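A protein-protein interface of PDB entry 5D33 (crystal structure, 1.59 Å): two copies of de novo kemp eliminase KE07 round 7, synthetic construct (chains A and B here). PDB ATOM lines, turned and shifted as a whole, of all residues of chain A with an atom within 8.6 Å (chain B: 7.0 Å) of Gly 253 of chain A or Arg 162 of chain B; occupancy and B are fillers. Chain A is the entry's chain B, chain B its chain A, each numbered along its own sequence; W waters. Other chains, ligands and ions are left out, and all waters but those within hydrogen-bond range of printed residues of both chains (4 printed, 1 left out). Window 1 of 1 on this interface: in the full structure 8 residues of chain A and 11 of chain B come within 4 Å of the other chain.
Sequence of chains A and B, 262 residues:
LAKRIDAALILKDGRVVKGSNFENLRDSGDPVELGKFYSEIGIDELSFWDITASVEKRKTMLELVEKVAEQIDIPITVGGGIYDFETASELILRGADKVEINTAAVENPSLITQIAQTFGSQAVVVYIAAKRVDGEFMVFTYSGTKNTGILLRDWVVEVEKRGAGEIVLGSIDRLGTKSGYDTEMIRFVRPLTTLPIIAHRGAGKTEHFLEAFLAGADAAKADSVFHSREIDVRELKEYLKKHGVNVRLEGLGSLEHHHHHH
The side-chain hydroxyl (OG) of Ser 110 of chain B is in hydrogen-bond range of the backbone carbonyl oxygen (O) of Leu 252 of chain A, at 2.7 Å. The guanidinium group (NH1) of Arg 162 of chain B is in hydrogen-bond range of the backbone carbonyl oxygen (O) of Leu 252 of chain A. The guanidinium group (NH2) of Arg 162 of chain B sits at hydrogen-bond distance from the backbone carbonyl oxygen (O) of Glu 250 of chain A. The backbone carbonyl oxygen (O) of Gly 253 of chain A is in hydrogen-bond range of the guanidinium group (NH1) of Arg 162 of chain B (3.3 Å). The side-chain hydroxyl (OG) of Ser 254 of chain A is in hydrogen-bond range of the guanidinium group (NH2) of Arg 162 of chain B (3.3 Å). The side-chain hydroxyl (OG) of Ser 121 of chain B sits close to a ring nitrogen (NE2) of His 258 of chain A (3.0 Å).
O of Gly 163 of chain B lies within hydrogen-bond range of OG of Ser 121 of chain B (2.9 Å). The backbone carbonyl oxygen (O) of Gly 251 of chain A sits at hydrogen-bond distance from the side-chain hydroxyl (OG) of Ser 254 of chain A. The side-chain hydroxyl of Ser 110 of chain B lies within hydrogen-bond range of the guanidinium group of Arg 162 of chain B (3.3 Å). A ring nitrogen (ND1) of His 257 of chain A sits at hydrogen-bond distance from the backbone NH of His 259 of chain A (3.1 Å).
Asn 108 of chain B touches Leu 249 of chain A. Glu 250 of chain A touches Pro 109 of chain B. OG of Ser 110 of chain B touches CA of Gly 253 of chain A, at 3.8 Å. His 257 of chain A touches Thr 113 of chain B. His 258 of chain A touches Thr 113 of chain B (N to CG2, 3.7 Å). CB of His 258 of chain A touches CB of Ala 116 of chain B (3.7 Å). O of His 258 of chain A touches CA of Gln 117 of chain B, 3.8 Å away. Arg 162 of chain B touches His 258 of chain A (O to ND1, 3.97 Å). CA of Gly 163 of chain B touches CE1 of His 258 of chain A (3.4 Å).
Glu 40 of chain A touches none of the printed residues of chain B. Of chain B, only Ser 110 (3.8 Å) and Arg 162 (3.3 Å) come within 4 Å of Gly 253 of chain A. Printed residues of chain A within 4 Å of Ser 110 of chain B: Leu 252 (2.7 Å) and Gly 253 (3.8 Å). Of the printed residues of chain A, Thr 113 of chain B touches His 257 (3.5 Å) and His 258 (3.7 Å). Glu 160 of chain B touches none of the printed residues of chain A. Of the printed residues of chain A, Arg 162 of chain B touches Glu 250, Leu 252, Gly 253, Ser 254 and His 258. Gly 163 of chain B touches just one residue of chain A: His 258 (3.4 Å). The nearest residue of chain B that does not touch Gly 253 of chain A is Thr 113 of chain B (5.4 Å). The nearest residue of chain A that does not touch Arg 162 of chain B is Gly 251 of chain A (4.6 Å).
Of the 19 printed residues of chain B, 9 touch a printed residue of chain A. Of the 18 printed residues of chain A, 7 touch a printed residue of chain B. Among the printed residues, 15 pairs touch across the chains. Among the printed residues, no Asp or Glu carboxylate lies within 4 Å of a Lys or Arg side-chain nitrogen of the other chain.
No position is printed for both chains.
Water W4 lies within hydrogen-bond range of OG1 of Thr 113 of chain B (2.7 Å), O of Gly 253 of chain A (2.7 Å) and NH1 of Arg 162 of chain B (2.9 Å). Water W2 lies within hydrogen-bond range of the backbone carbonyl oxygen of Glu 250 of chain A (2.8 Å), the guanidinium group of Arg 162 of chain B (3.3 Å) and the side-chain carboxylate of Glu 158 of chain B (3.5 Å).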
ATOM      1  N   PHE A  37       4.380  13.637   4.458  1.00  0.00           N
ATOM      2  CA  PHE A  37       4.212  12.485   3.585  1.00  0.00           C
ATOM      3  C   PHE A  37       5.486  11.648   3.507  1.00  0.00           C
ATOM      4  O   PHE A  37       5.444  10.417   3.604  1.00  0.00           O
ATOM      5  CB  PHE A  37       3.771  12.965   2.202  1.00  0.00           C
ATOM      6  CG  PHE A  37       3.750  11.897   1.161  1.00  0.00           C
ATOM      7  CD1 PHE A  37       2.775  10.906   1.166  1.00  0.00           C
ATOM      8  CD2 PHE A  37       4.696  11.897   0.152  1.00  0.00           C
ATOM      9  CE1 PHE A  37       2.761   9.929   0.180  1.00  0.00           C
ATOM     10  CE2 PHE A  37       4.684  10.925  -0.838  1.00  0.00           C
ATOM     11  CZ  PHE A  37       3.713   9.944  -0.823  1.00  0.00           C
ATOM     12  N   SER A  39       7.680  11.463   5.783  1.00  0.00           N
ATOM     13  CA  SER A  39       7.866  10.816   7.082  1.00  0.00           C
ATOM     14  C   SER A  39       6.972   9.589   7.208  1.00  0.00           C
ATOM     15  O   SER A  39       7.202   8.722   8.050  1.00  0.00           O
ATOM     16  CB  SER A  39       7.571  11.794   8.220  1.00  0.00           C
ATOM     17  OG  SER A  39       6.177  11.899   8.453  1.00  0.00           O
ATOM     18  N   GLU A  40       5.944   9.505   6.374  1.00  0.00           N
ATOM     19  CA  GLU A  40       5.045   8.363   6.472  1.00  0.00           C
ATOM     20  C   GLU A  40       5.225   7.350   5.344  1.00  0.00           C
ATOM     21  O   GLU A  40       4.435   6.422   5.215  1.00  0.00           O
ATOM     22  CB  GLU A  40       3.605   8.854   6.552  1.00  0.00           C
ATOM     23  CG  GLU A  40       3.370   9.719   7.781  1.00  0.00           C
ATOM     24  CD  GLU A  40       1.921  10.088   7.986  1.00  0.00           C
ATOM     25  OE1 GLU A  40       1.402  10.918   7.209  1.00  0.00           O
ATOM     26  OE2 GLU A  40       1.301   9.547   8.929  1.00  0.00           O
ATOM     27  N   ILE A  41       6.292   7.485   4.556  1.00  0.00           N
ATOM     28  CA  ILE A  41       6.573   6.475   3.537  1.00  0.00           C
ATOM     29  C   ILE A  41       7.989   5.885   3.644  1.00  0.00           C
ATOM     30  O   ILE A  41       8.360   5.012   2.866  1.00  0.00           O
ATOM     31  CB  ILE A  41       6.374   7.026   2.109  1.00  0.00           C
ATOM     32  CG1 ILE A  41       7.380   8.156   1.825  1.00  0.00           C
ATOM     33  CG2 ILE A  41       4.915   7.446   1.892  1.00  0.00           C
ATOM     34  CD1 ILE A  41       7.397   8.546   0.340  1.00  0.00           C
ATOM     35  N   GLY A  42       8.780   6.322   4.619  1.00  0.00           N
ATOM     36  CA  GLY A  42      10.083   5.711   4.788  1.00  0.00           C
ATOM     37  C   GLY A  42      11.289   6.631   4.873  1.00  0.00           C
ATOM     38  O   GLY A  42      12.402   6.164   5.051  1.00  0.00           O
ATOM     39  N   ARG A 234      10.290   3.839  -0.738  1.00  0.00           N
ATOM     40  CA  ARG A 234      10.079   2.468  -0.279  1.00  0.00           C
ATOM     41  C   ARG A 234      10.921   1.477  -1.085  1.00  0.00           C
ATOM     42  O   ARG A 234      11.507   0.567  -0.512  1.00  0.00           O
ATOM     43  CB  ARG A 234       8.588   2.111  -0.345  1.00  0.00           C
ATOM     44  CG  ARG A 234       8.240   0.928  -1.227  1.00  0.00           C
ATOM     45  CD  ARG A 234       6.736   0.826  -1.399  1.00  0.00           C
ATOM     46  NE  ARG A 234       6.132   0.224  -0.224  1.00  0.00           N
ATOM     47  CZ  ARG A 234       4.841   0.265   0.074  1.00  0.00           C
ATOM     48  NH1 ARG A 234       3.979   0.909  -0.707  1.00  0.00           N
ATOM     49  NH2 ARG A 234       4.417  -0.332   1.176  1.00  0.00           N
ATOM     50  N   GLU A 238      13.783  -1.022   0.411  1.00  0.00           N
ATOM     51  CA  GLU A 238      13.679  -2.459   0.167  1.00  0.00           C
ATOM     52  C   GLU A 238      14.917  -3.001  -0.561  1.00  0.00           C
ATOM     53  O   GLU A 238      15.407  -4.088  -0.230  1.00  0.00           O
ATOM     54  CB  GLU A 238      12.398  -2.769  -0.617  1.00  0.00           C
ATOM     55  CG  GLU A 238      11.127  -2.639   0.251  1.00  0.00           C
ATOM     56  CD  GLU A 238       9.838  -2.853  -0.501  1.00  0.00           C
ATOM     57  OE1 GLU A 238       9.833  -2.732  -1.742  1.00  0.00           O
ATOM     58  OE2 GLU A 238       8.816  -3.128   0.165  1.00  0.00           O
ATOM     59  N   LEU A 249      12.861   0.038   8.492  1.00  0.00           N
ATOM     60  CA  LEU A 249      11.649  -0.209   7.715  1.00  0.00           C
ATOM     61  C   LEU A 249      10.382   0.199   8.454  1.00  0.00           C
ATOM     62  O   LEU A 249       9.297  -0.031   7.944  1.00  0.00           O
ATOM     63  CB  LEU A 249      11.533  -1.694   7.353  1.00  0.00           C
ATOM     64  CG  LEU A 249      12.763  -2.386   6.768  1.00  0.00           C
ATOM     65  CD1 LEU A 249      12.518  -3.893   6.670  1.00  0.00           C
ATOM     66  CD2 LEU A 249      13.089  -1.810   5.424  1.00  0.00           C
ATOM     67  N   GLU A 250      10.515   0.772   9.655  1.00  0.00           N
ATOM     68  CA  GLU A 250       9.345   1.031  10.502  1.00  0.00           C
ATOM     69  C   GLU A 250       8.359   2.015   9.879  1.00  0.00           C
ATOM     70  O   GLU A 250       7.158   1.981  10.179  1.00  0.00           O
ATOM     71  CB  GLU A 250       9.763   1.558  11.882  1.00  0.00           C
ATOM     72  CG  GLU A 250      10.456   0.540  12.780  1.00  0.00           C
ATOM     73  CD  GLU A 250      11.945   0.413  12.496  1.00  0.00           C
ATOM     74  OE1 GLU A 250      12.446   1.122  11.600  1.00  0.00           O
ATOM     75  OE2 GLU A 250      12.619  -0.392  13.174  1.00  0.00           O
ATOM     76  N   GLY A 251       8.870   2.913   9.046  1.00  0.00           N
ATOM     77  CA  GLY A 251       8.047   3.972   8.479  1.00  0.00           C
ATOM     78  C   GLY A 251       7.337   3.571   7.196  1.00  0.00           C
ATOM     79  O   GLY A 251       6.404   4.255   6.756  1.00  0.00           O
ATOM     80  N   LEU A 252       7.773   2.462   6.608  1.00  0.00           N
ATOM     81  CA  LEU A 252       7.176   1.941   5.396  1.00  0.00           C
ATOM     82  C   LEU A 252       5.711   1.574   5.608  1.00  0.00           C
ATOM     83  O   LEU A 252       5.348   0.960   6.610  1.00  0.00           O
ATOM     84  CB  LEU A 252       7.938   0.710   4.886  1.00  0.00           C
ATOM     85  CG  LEU A 252       9.414   0.844   4.515  1.00  0.00           C
ATOM     86  CD1 LEU A 252       9.868  -0.364   3.691  1.00  0.00           C
ATOM     87  CD2 LEU A 252       9.626   2.115   3.758  1.00  0.00           C
ATOM     88  N   GLY A 253       4.880   1.951   4.647  1.00  0.00           N
ATOM     89  CA  GLY A 253       3.479   1.555   4.630  1.00  0.00           C
ATOM     90  C   GLY A 253       2.593   2.207   5.670  1.00  0.00           C
ATOM     91  O   GLY A 253       1.499   1.718   5.918  1.00  0.00           O
ATOM     92  N   SER A 254       3.045   3.302   6.272  1.00  0.00           N
ATOM     93  CA  SER A 254       2.284   3.926   7.357  1.00  0.00           C
ATOM     94  C   SER A 254       0.941   4.452   6.858  1.00  0.00           C
ATOM     95  O   SER A 254      -0.018   4.565   7.618  1.00  0.00           O
ATOM     96  CB  SER A 254       3.076   5.070   7.993  1.00  0.00           C
ATOM     97  OG  SER A 254       4.258   4.601   8.631  1.00  0.00           O
ATOM     98  N   LEU A 255       0.876   4.773   5.571  1.00  0.00           N
ATOM     99  CA  LEU A 255      -0.358   5.277   4.981  1.00  0.00           C
ATOM    100  C   LEU A 255      -1.285   4.177   4.462  1.00  0.00           C
ATOM    101  O   LEU A 255      -2.424   4.455   4.083  1.00  0.00           O
ATOM    102  CB  LEU A 255      -0.040   6.257   3.851  1.00  0.00           C
ATOM    103  CG  LEU A 255       0.868   7.425   4.224  1.00  0.00           C
ATOM    104  CD1 LEU A 255       1.122   8.283   2.995  1.00  0.00           C
ATOM    105  CD2 LEU A 255       0.253   8.244   5.350  1.00  0.00           C
ATOM    106  N   GLU A 256      -0.825   2.929   4.472  1.00  0.00           N
ATOM    107  CA  GLU A 256      -1.616   1.845   3.893  1.00  0.00           C
ATOM    108  C   GLU A 256      -2.384   1.111   4.964  1.00  0.00           C
ATOM    109  O   GLU A 256      -2.049   1.177   6.141  1.00  0.00           O
ATOM    110  CB  GLU A 256      -0.722   0.882   3.116  1.00  0.00           C
ATOM    111  CG  GLU A 256       0.061   1.619   2.041  1.00  0.00           C
ATOM    112  CD  GLU A 256       1.219   0.830   1.461  1.00  0.00           C
ATOM    113  OE1 GLU A 256       1.528  -0.272   1.963  1.00  0.00           O
ATOM    114  OE2 GLU A 256       1.828   1.328   0.489  1.00  0.00           O
ATOM    115  N   HIS A 257      -3.434   0.416   4.550  1.00  0.00           N
ATOM    116  CA  HIS A 257      -4.323  -0.225   5.506  1.00  0.00           C
ATOM    117  C   HIS A 257      -4.739  -1.587   4.982  1.00  0.00           C
ATOM    118  O   HIS A 257      -4.421  -1.956   3.848  1.00  0.00           O
ATOM    119  CB  HIS A 257      -5.550   0.655   5.781  1.00  0.00           C
ATOM    120  CG  HIS A 257      -6.290   1.045   4.539  1.00  0.00           C
ATOM    121  ND1 HIS A 257      -7.076   0.158   3.835  1.00  0.00           N
ATOM    122  CD2 HIS A 257      -6.353   2.220   3.866  1.00  0.00           C
ATOM    123  CE1 HIS A 257      -7.594   0.770   2.785  1.00  0.00           C
ATOM    124  NE2 HIS A 257      -7.166   2.020   2.777  1.00  0.00           N
ATOM    125  N   HIS A 258      -5.457  -2.338   5.810  1.00  0.00           N
ATOM    126  CA  HIS A 258      -5.795  -3.712   5.470  1.00  0.00           C
ATOM    127  C   HIS A 258      -7.210  -3.850   4.928  1.00  0.00           C
ATOM    128  O   HIS A 258      -7.745  -4.952   4.868  1.00  0.00           O
ATOM    129  CB  HIS A 258      -5.623  -4.621   6.693  1.00  0.00           C
ATOM    130  CG  HIS A 258      -6.420  -4.195   7.893  1.00  0.00           C
ATOM    131  ND1 HIS A 258      -6.188  -3.011   8.558  1.00  0.00           N
ATOM    132  CD2 HIS A 258      -7.434  -4.804   8.552  1.00  0.00           C
ATOM    133  CE1 HIS A 258      -7.025  -2.908   9.576  1.00  0.00           C
ATOM    134  NE2 HIS A 258      -7.791  -3.984   9.596  1.00  0.00           N
ATOM    135  N   HIS A 259      -7.821  -2.729   4.551  1.00  0.00           N
ATOM    136  CA  HIS A 259      -9.137  -2.755   3.940  1.00  0.00           C
ATOM    137  C   HIS A 259      -9.003  -2.546   2.445  1.00  0.00           C
ATOM    138  O   HIS A 259      -7.897  -2.420   1.918  1.00  0.00           O
ATOM    139  CB  HIS A 259     -10.032  -1.683   4.542  1.00  0.00           C
ATOM    140  CG  HIS A 259      -9.963  -1.625   6.035  1.00  0.00           C
ATOM    141  ND1 HIS A 259     -10.530  -2.590   6.840  1.00  0.00           N
ATOM    142  CD2 HIS A 259      -9.378  -0.734   6.869  1.00  0.00           C
ATOM    143  CE1 HIS A 259     -10.309  -2.286   8.106  1.00  0.00           C
ATOM    144  NE2 HIS A 259      -9.613  -1.165   8.152  1.00  0.00           N
ATOM    145  N   ASN B 108       9.228  -4.358  10.925  1.00  0.00           N
ATOM    146  CA  ASN B 108       8.562  -4.147   9.659  1.00  0.00           C
ATOM    147  C   ASN B 108       7.069  -4.233   9.918  1.00  0.00           C
ATOM    148  O   ASN B 108       6.444  -5.246   9.604  1.00  0.00           O
ATOM    149  CB  ASN B 108       9.016  -5.194   8.640  1.00  0.00           C
ATOM    150  CG  ASN B 108       8.455  -4.956   7.244  1.00  0.00           C
ATOM    151  OD1 ASN B 108       8.189  -3.826   6.850  1.00  0.00           O
ATOM    152  ND2 ASN B 108       8.282  -6.032   6.494  1.00  0.00           N
ATOM    153  N   PRO B 109       6.503  -3.191  10.533  1.00  0.00           N
ATOM    154  CA  PRO B 109       5.078  -3.223  10.898  1.00  0.00           C
ATOM    155  C   PRO B 109       4.143  -3.405   9.696  1.00  0.00           C
ATOM    156  O   PRO B 109       3.012  -3.870   9.886  1.00  0.00           O
ATOM    157  CB  PRO B 109       4.842  -1.872  11.580  1.00  0.00           C
ATOM    158  CG  PRO B 109       6.074  -1.077  11.372  1.00  0.00           C
ATOM    159  CD  PRO B 109       7.191  -1.994  11.046  1.00  0.00           C
ATOM    160  N   SER B 110       4.610  -3.073   8.488  1.00  0.00           N
ATOM    161  CA  SER B 110       3.882  -3.383   7.257  1.00  0.00           C
ATOM    162  C   SER B 110       3.461  -4.831   7.148  1.00  0.00           C
ATOM    163  O   SER B 110       2.469  -5.140   6.512  1.00  0.00           O
ATOM    164  CB  SER B 110       4.737  -3.053   6.033  1.00  0.00           C
ATOM    165  OG  SER B 110       4.926  -1.655   5.948  1.00  0.00           O
ATOM    166  N   LEU B 111       4.253  -5.723   7.735  1.00  0.00           N
ATOM    167  CA  LEU B 111       3.938  -7.140   7.679  1.00  0.00           C
ATOM    168  C   LEU B 111       2.570  -7.483   8.291  1.00  0.00           C
ATOM    169  O   LEU B 111       1.875  -8.380   7.801  1.00  0.00           O
ATOM    170  CB  LEU B 111       5.034  -7.927   8.387  1.00  0.00           C
ATOM    171  CG  LEU B 111       4.794  -9.431   8.545  1.00  0.00           C
ATOM    172  CD1 LEU B 111       4.643 -10.124   7.204  1.00  0.00           C
ATOM    173  CD2 LEU B 111       5.916 -10.069   9.343  1.00  0.00           C
ATOM    174  N   ILE B 112       2.202  -6.777   9.361  1.00  0.00           N
ATOM    175  CA  ILE B 112       0.907  -6.952  10.006  1.00  0.00           C
ATOM    176  C   ILE B 112      -0.161  -6.693   8.990  1.00  0.00           C
ATOM    177  O   ILE B 112      -1.065  -7.503   8.779  1.00  0.00           O
ATOM    178  CB  ILE B 112       0.710  -5.986  11.174  1.00  0.00           C
ATOM    179  CG1 ILE B 112       1.723  -6.312  12.268  1.00  0.00           C
ATOM    180  CG2 ILE B 112      -0.716  -6.054  11.655  1.00  0.00           C
ATOM    181  CD1 ILE B 112       1.818  -5.237  13.333  1.00  0.00           C
ATOM    182  N   THR B 113      -0.009  -5.565   8.312  1.00  0.00           N
ATOM    183  CA  THR B 113      -0.984  -5.162   7.332  1.00  0.00           C
ATOM    184  C   THR B 113      -1.043  -6.097   6.130  1.00  0.00           C
ATOM    185  O   THR B 113      -2.121  -6.367   5.614  1.00  0.00           O
ATOM    186  CB  THR B 113      -0.694  -3.734   6.829  1.00  0.00           C
ATOM    187  OG1 THR B 113      -0.482  -2.861   7.938  1.00  0.00           O
ATOM    188  CG2 THR B 113      -1.865  -3.218   5.995  1.00  0.00           C
ATOM    189  N   GLN B 114       0.110  -6.605   5.697  1.00  0.00           N
ATOM    190  CA  GLN B 114       0.129  -7.476   4.532  1.00  0.00           C
ATOM    191  C   GLN B 114      -0.660  -8.741   4.814  1.00  0.00           C
ATOM    192  O   GLN B 114      -1.448  -9.177   3.970  1.00  0.00           O
ATOM    193  CB  GLN B 114       1.554  -7.830   4.137  1.00  0.00           C
ATOM    194  CG  GLN B 114       2.384  -6.648   3.766  1.00  0.00           C
ATOM    195  CD  GLN B 114       3.850  -7.004   3.690  1.00  0.00           C
ATOM    196  OE1 GLN B 114       4.206  -8.180   3.614  1.00  0.00           O
ATOM    197  NE2 GLN B 114       4.711  -5.992   3.727  1.00  0.00           N
ATOM    198  N   ALA B 116      -2.965  -9.200   7.250  1.00  0.00           N
ATOM    199  CA  ALA B 116      -4.370  -8.842   7.465  1.00  0.00           C
ATOM    200  C   ALA B 116      -5.128  -8.509   6.172  1.00  0.00           C
ATOM    201  O   ALA B 116      -6.329  -8.744   6.066  1.00  0.00           O
ATOM    202  CB  ALA B 116      -4.469  -7.664   8.449  1.00  0.00           C
ATOM    203  N   GLN B 117      -4.435  -7.963   5.189  1.00  0.00           N
ATOM    204  CA  GLN B 117      -5.106  -7.508   3.985  1.00  0.00           C
ATOM    205  C   GLN B 117      -5.625  -8.684   3.162  1.00  0.00           C
ATOM    206  O   GLN B 117      -6.621  -8.560   2.443  1.00  0.00           O
ATOM    207  CB  GLN B 117      -4.158  -6.653   3.154  1.00  0.00           C
ATOM    208  CG  GLN B 117      -4.762  -6.054   1.906  1.00  0.00           C
ATOM    209  CD  GLN B 117      -3.717  -5.338   1.081  1.00  0.00           C
ATOM    210  OE1 GLN B 117      -2.574  -5.166   1.520  1.00  0.00           O
ATOM    211  NE2 GLN B 117      -4.094  -4.921  -0.119  1.00  0.00           N
ATOM    212  N   SER B 121      -7.866  -9.460   9.681  1.00  0.00           N
ATOM    213  CA  SER B 121      -7.222  -9.122  10.946  1.00  0.00           C
ATOM    214  C   SER B 121      -7.268 -10.285  11.924  1.00  0.00           C
ATOM    215  O   SER B 121      -6.343 -10.478  12.704  1.00  0.00           O
ATOM    216  CB  SER B 121      -7.884  -7.900  11.582  1.00  0.00           C
ATOM    217  OG  SER B 121      -7.687  -6.749  10.791  1.00  0.00           O
ATOM    218  N   TRP B 155       3.678   1.087  20.772  1.00  0.00           N
ATOM    219  CA  TRP B 155       3.625  -0.068  19.896  1.00  0.00           C
ATOM    220  C   TRP B 155       2.231  -0.697  19.898  1.00  0.00           C
ATOM    221  O   TRP B 155       1.754  -1.137  18.866  1.00  0.00           O
ATOM    222  CB  TRP B 155       4.719  -1.078  20.290  1.00  0.00           C
ATOM    223  CG  TRP B 155       4.779  -2.327  19.446  1.00  0.00           C
ATOM    224  CD1 TRP B 155       4.876  -3.607  19.910  1.00  0.00           C
ATOM    225  CD2 TRP B 155       4.755  -2.422  18.006  1.00  0.00           C
ATOM    226  NE1 TRP B 155       4.914  -4.491  18.864  1.00  0.00           N
ATOM    227  CE2 TRP B 155       4.868  -3.796  17.683  1.00  0.00           C
ATOM    228  CE3 TRP B 155       4.694  -1.486  16.970  1.00  0.00           C
ATOM    229  CZ2 TRP B 155       4.856  -4.263  16.366  1.00  0.00           C
ATOM    230  CZ3 TRP B 155       4.678  -1.949  15.648  1.00  0.00           C
ATOM    231  CH2 TRP B 155       4.776  -3.332  15.362  1.00  0.00           C
ATOM    232  N   VAL B 157      -0.625   0.840  20.144  1.00  0.00           N
ATOM    233  CA  VAL B 157      -1.452   1.672  19.300  1.00  0.00           C
ATOM    234  C   VAL B 157      -1.135   1.413  17.814  1.00  0.00           C
ATOM    235  O   VAL B 157      -2.052   1.315  16.980  1.00  0.00           O
ATOM    236  CB  VAL B 157      -1.269   3.170  19.660  1.00  0.00           C
ATOM    237  CG1 VAL B 157      -1.924   4.065  18.609  1.00  0.00           C
ATOM    238  CG2 VAL B 157      -1.855   3.451  21.038  1.00  0.00           C
ATOM    239  N   GLU B 158       0.148   1.251  17.489  1.00  0.00           N
ATOM    240  CA  GLU B 158       0.536   1.025  16.091  1.00  0.00           C
ATOM    241  C   GLU B 158       0.083  -0.354  15.613  1.00  0.00           C
ATOM    242  O   GLU B 158      -0.357  -0.515  14.463  1.00  0.00           O
ATOM    243  CB  GLU B 158       2.043   1.171  15.907  1.00  0.00           C
ATOM    244  CG  GLU B 158       2.489   1.042  14.455  1.00  0.00           C
ATOM    245  CD  GLU B 158       2.200   2.281  13.633  1.00  0.00           C
ATOM    246  OE1 GLU B 158       2.076   3.385  14.206  1.00  0.00           O
ATOM    247  OE2 GLU B 158       2.116   2.146  12.397  1.00  0.00           O
ATOM    248  N   VAL B 159       0.172  -1.335  16.504  1.00  0.00           N
ATOM    249  CA  VAL B 159      -0.248  -2.691  16.191  1.00  0.00           C
ATOM    250  C   VAL B 159      -1.717  -2.741  15.782  1.00  0.00           C
ATOM    251  O   VAL B 159      -2.061  -3.412  14.834  1.00  0.00           O
ATOM    252  CB  VAL B 159       0.039  -3.620  17.404  1.00  0.00           C
ATOM    253  CG1 VAL B 159      -0.645  -4.964  17.291  1.00  0.00           C
ATOM    254  CG2 VAL B 159       1.525  -3.818  17.512  1.00  0.00           C
ATOM    255  N   GLU B 160      -2.584  -2.038  16.506  1.00  0.00           N
ATOM    256  CA  GLU B 160      -3.984  -2.011  16.151  1.00  0.00           C
ATOM    257  C   GLU B 160      -4.181  -1.249  14.836  1.00  0.00           C
ATOM    258  O   GLU B 160      -4.910  -1.716  13.973  1.00  0.00           O
ATOM    259  CB  GLU B 160      -4.829  -1.389  17.280  1.00  0.00           C
ATOM    260  CG  GLU B 160      -6.320  -1.278  16.918  1.00  0.00           C
ATOM    261  CD  GLU B 160      -7.228  -0.865  18.082  1.00  0.00           C
ATOM    262  OE1 GLU B 160      -6.759  -0.737  19.222  1.00  0.00           O
ATOM    263  OE2 GLU B 160      -8.430  -0.656  17.834  1.00  0.00           O
ATOM    264  N   LYS B 161      -3.496  -0.110  14.690  1.00  0.00           N
ATOM    265  CA  LYS B 161      -3.587   0.694  13.477  1.00  0.00           C
ATOM    266  C   LYS B 161      -3.200  -0.084  12.222  1.00  0.00           C
ATOM    267  O   LYS B 161      -3.838   0.051  11.182  1.00  0.00           O
ATOM    268  CB  LYS B 161      -2.701   1.930  13.609  1.00  0.00           C
ATOM    269  CG  LYS B 161      -2.679   2.807  12.370  1.00  0.00           C
ATOM    270  CD  LYS B 161      -1.718   3.977  12.587  1.00  0.00           C
ATOM    271  CE  LYS B 161      -1.597   4.853  11.351  1.00  0.00           C
ATOM    272  NZ  LYS B 161      -0.583   5.926  11.535  1.00  0.00           N
ATOM    273  N   ARG B 162      -2.154  -0.895  12.329  1.00  0.00           N
ATOM    274  CA  ARG B 162      -1.712  -1.699  11.187  1.00  0.00           C
ATOM    275  C   ARG B 162      -2.649  -2.857  10.859  1.00  0.00           C
ATOM    276  O   ARG B 162      -2.470  -3.513   9.846  1.00  0.00           O
ATOM    277  CB  ARG B 162      -0.302  -2.248  11.443  1.00  0.00           C
ATOM    278  CG  ARG B 162       0.763  -1.157  11.578  1.00  0.00           C
ATOM    279  CD  ARG B 162       1.227  -0.695  10.201  1.00  0.00           C
ATOM    280  NE  ARG B 162       2.296   0.294  10.343  1.00  0.00           N
ATOM    281  CZ  ARG B 162       3.203   0.583   9.409  1.00  0.00           C
ATOM    282  NH1 ARG B 162       3.177  -0.017   8.220  1.00  0.00           N
ATOM    283  NH2 ARG B 162       4.136   1.480   9.667  1.00  0.00           N
ATOM    284  N   GLY B 163      -3.623  -3.157  11.717  1.00  0.00           N
ATOM    285  CA  GLY B 163      -4.544  -4.236  11.394  1.00  0.00           C
ATOM    286  C   GLY B 163      -4.407  -5.583  12.091  1.00  0.00           C
ATOM    287  O   GLY B 163      -4.903  -6.588  11.588  1.00  0.00           O
ATOM    288  N   ALA B 164      -3.771  -5.629  13.255  1.00  0.00           N
ATOM    289  CA  ALA B 164      -3.691  -6.885  14.009  1.00  0.00           C
ATOM    290  C   ALA B 164      -5.037  -7.251  14.637  1.00  0.00           C
ATOM    291  O   ALA B 164      -5.851  -6.381  14.952  1.00  0.00           O
ATOM    292  CB  ALA B 164      -2.613  -6.806  15.082  1.00  0.00           C
HETATM  293  O   HOH W   1      -4.725  -0.683   8.684  1.00  0.00           O
HETATM  294  O   HOH W   2       5.581   2.451  12.462  1.00  0.00           O
HETATM  295  O   HOH W   3      -0.459   7.080   8.912  1.00  0.00           O
HETATM  296  O   HOH W   4       0.854  -0.841   6.683  1.00  0.00           O
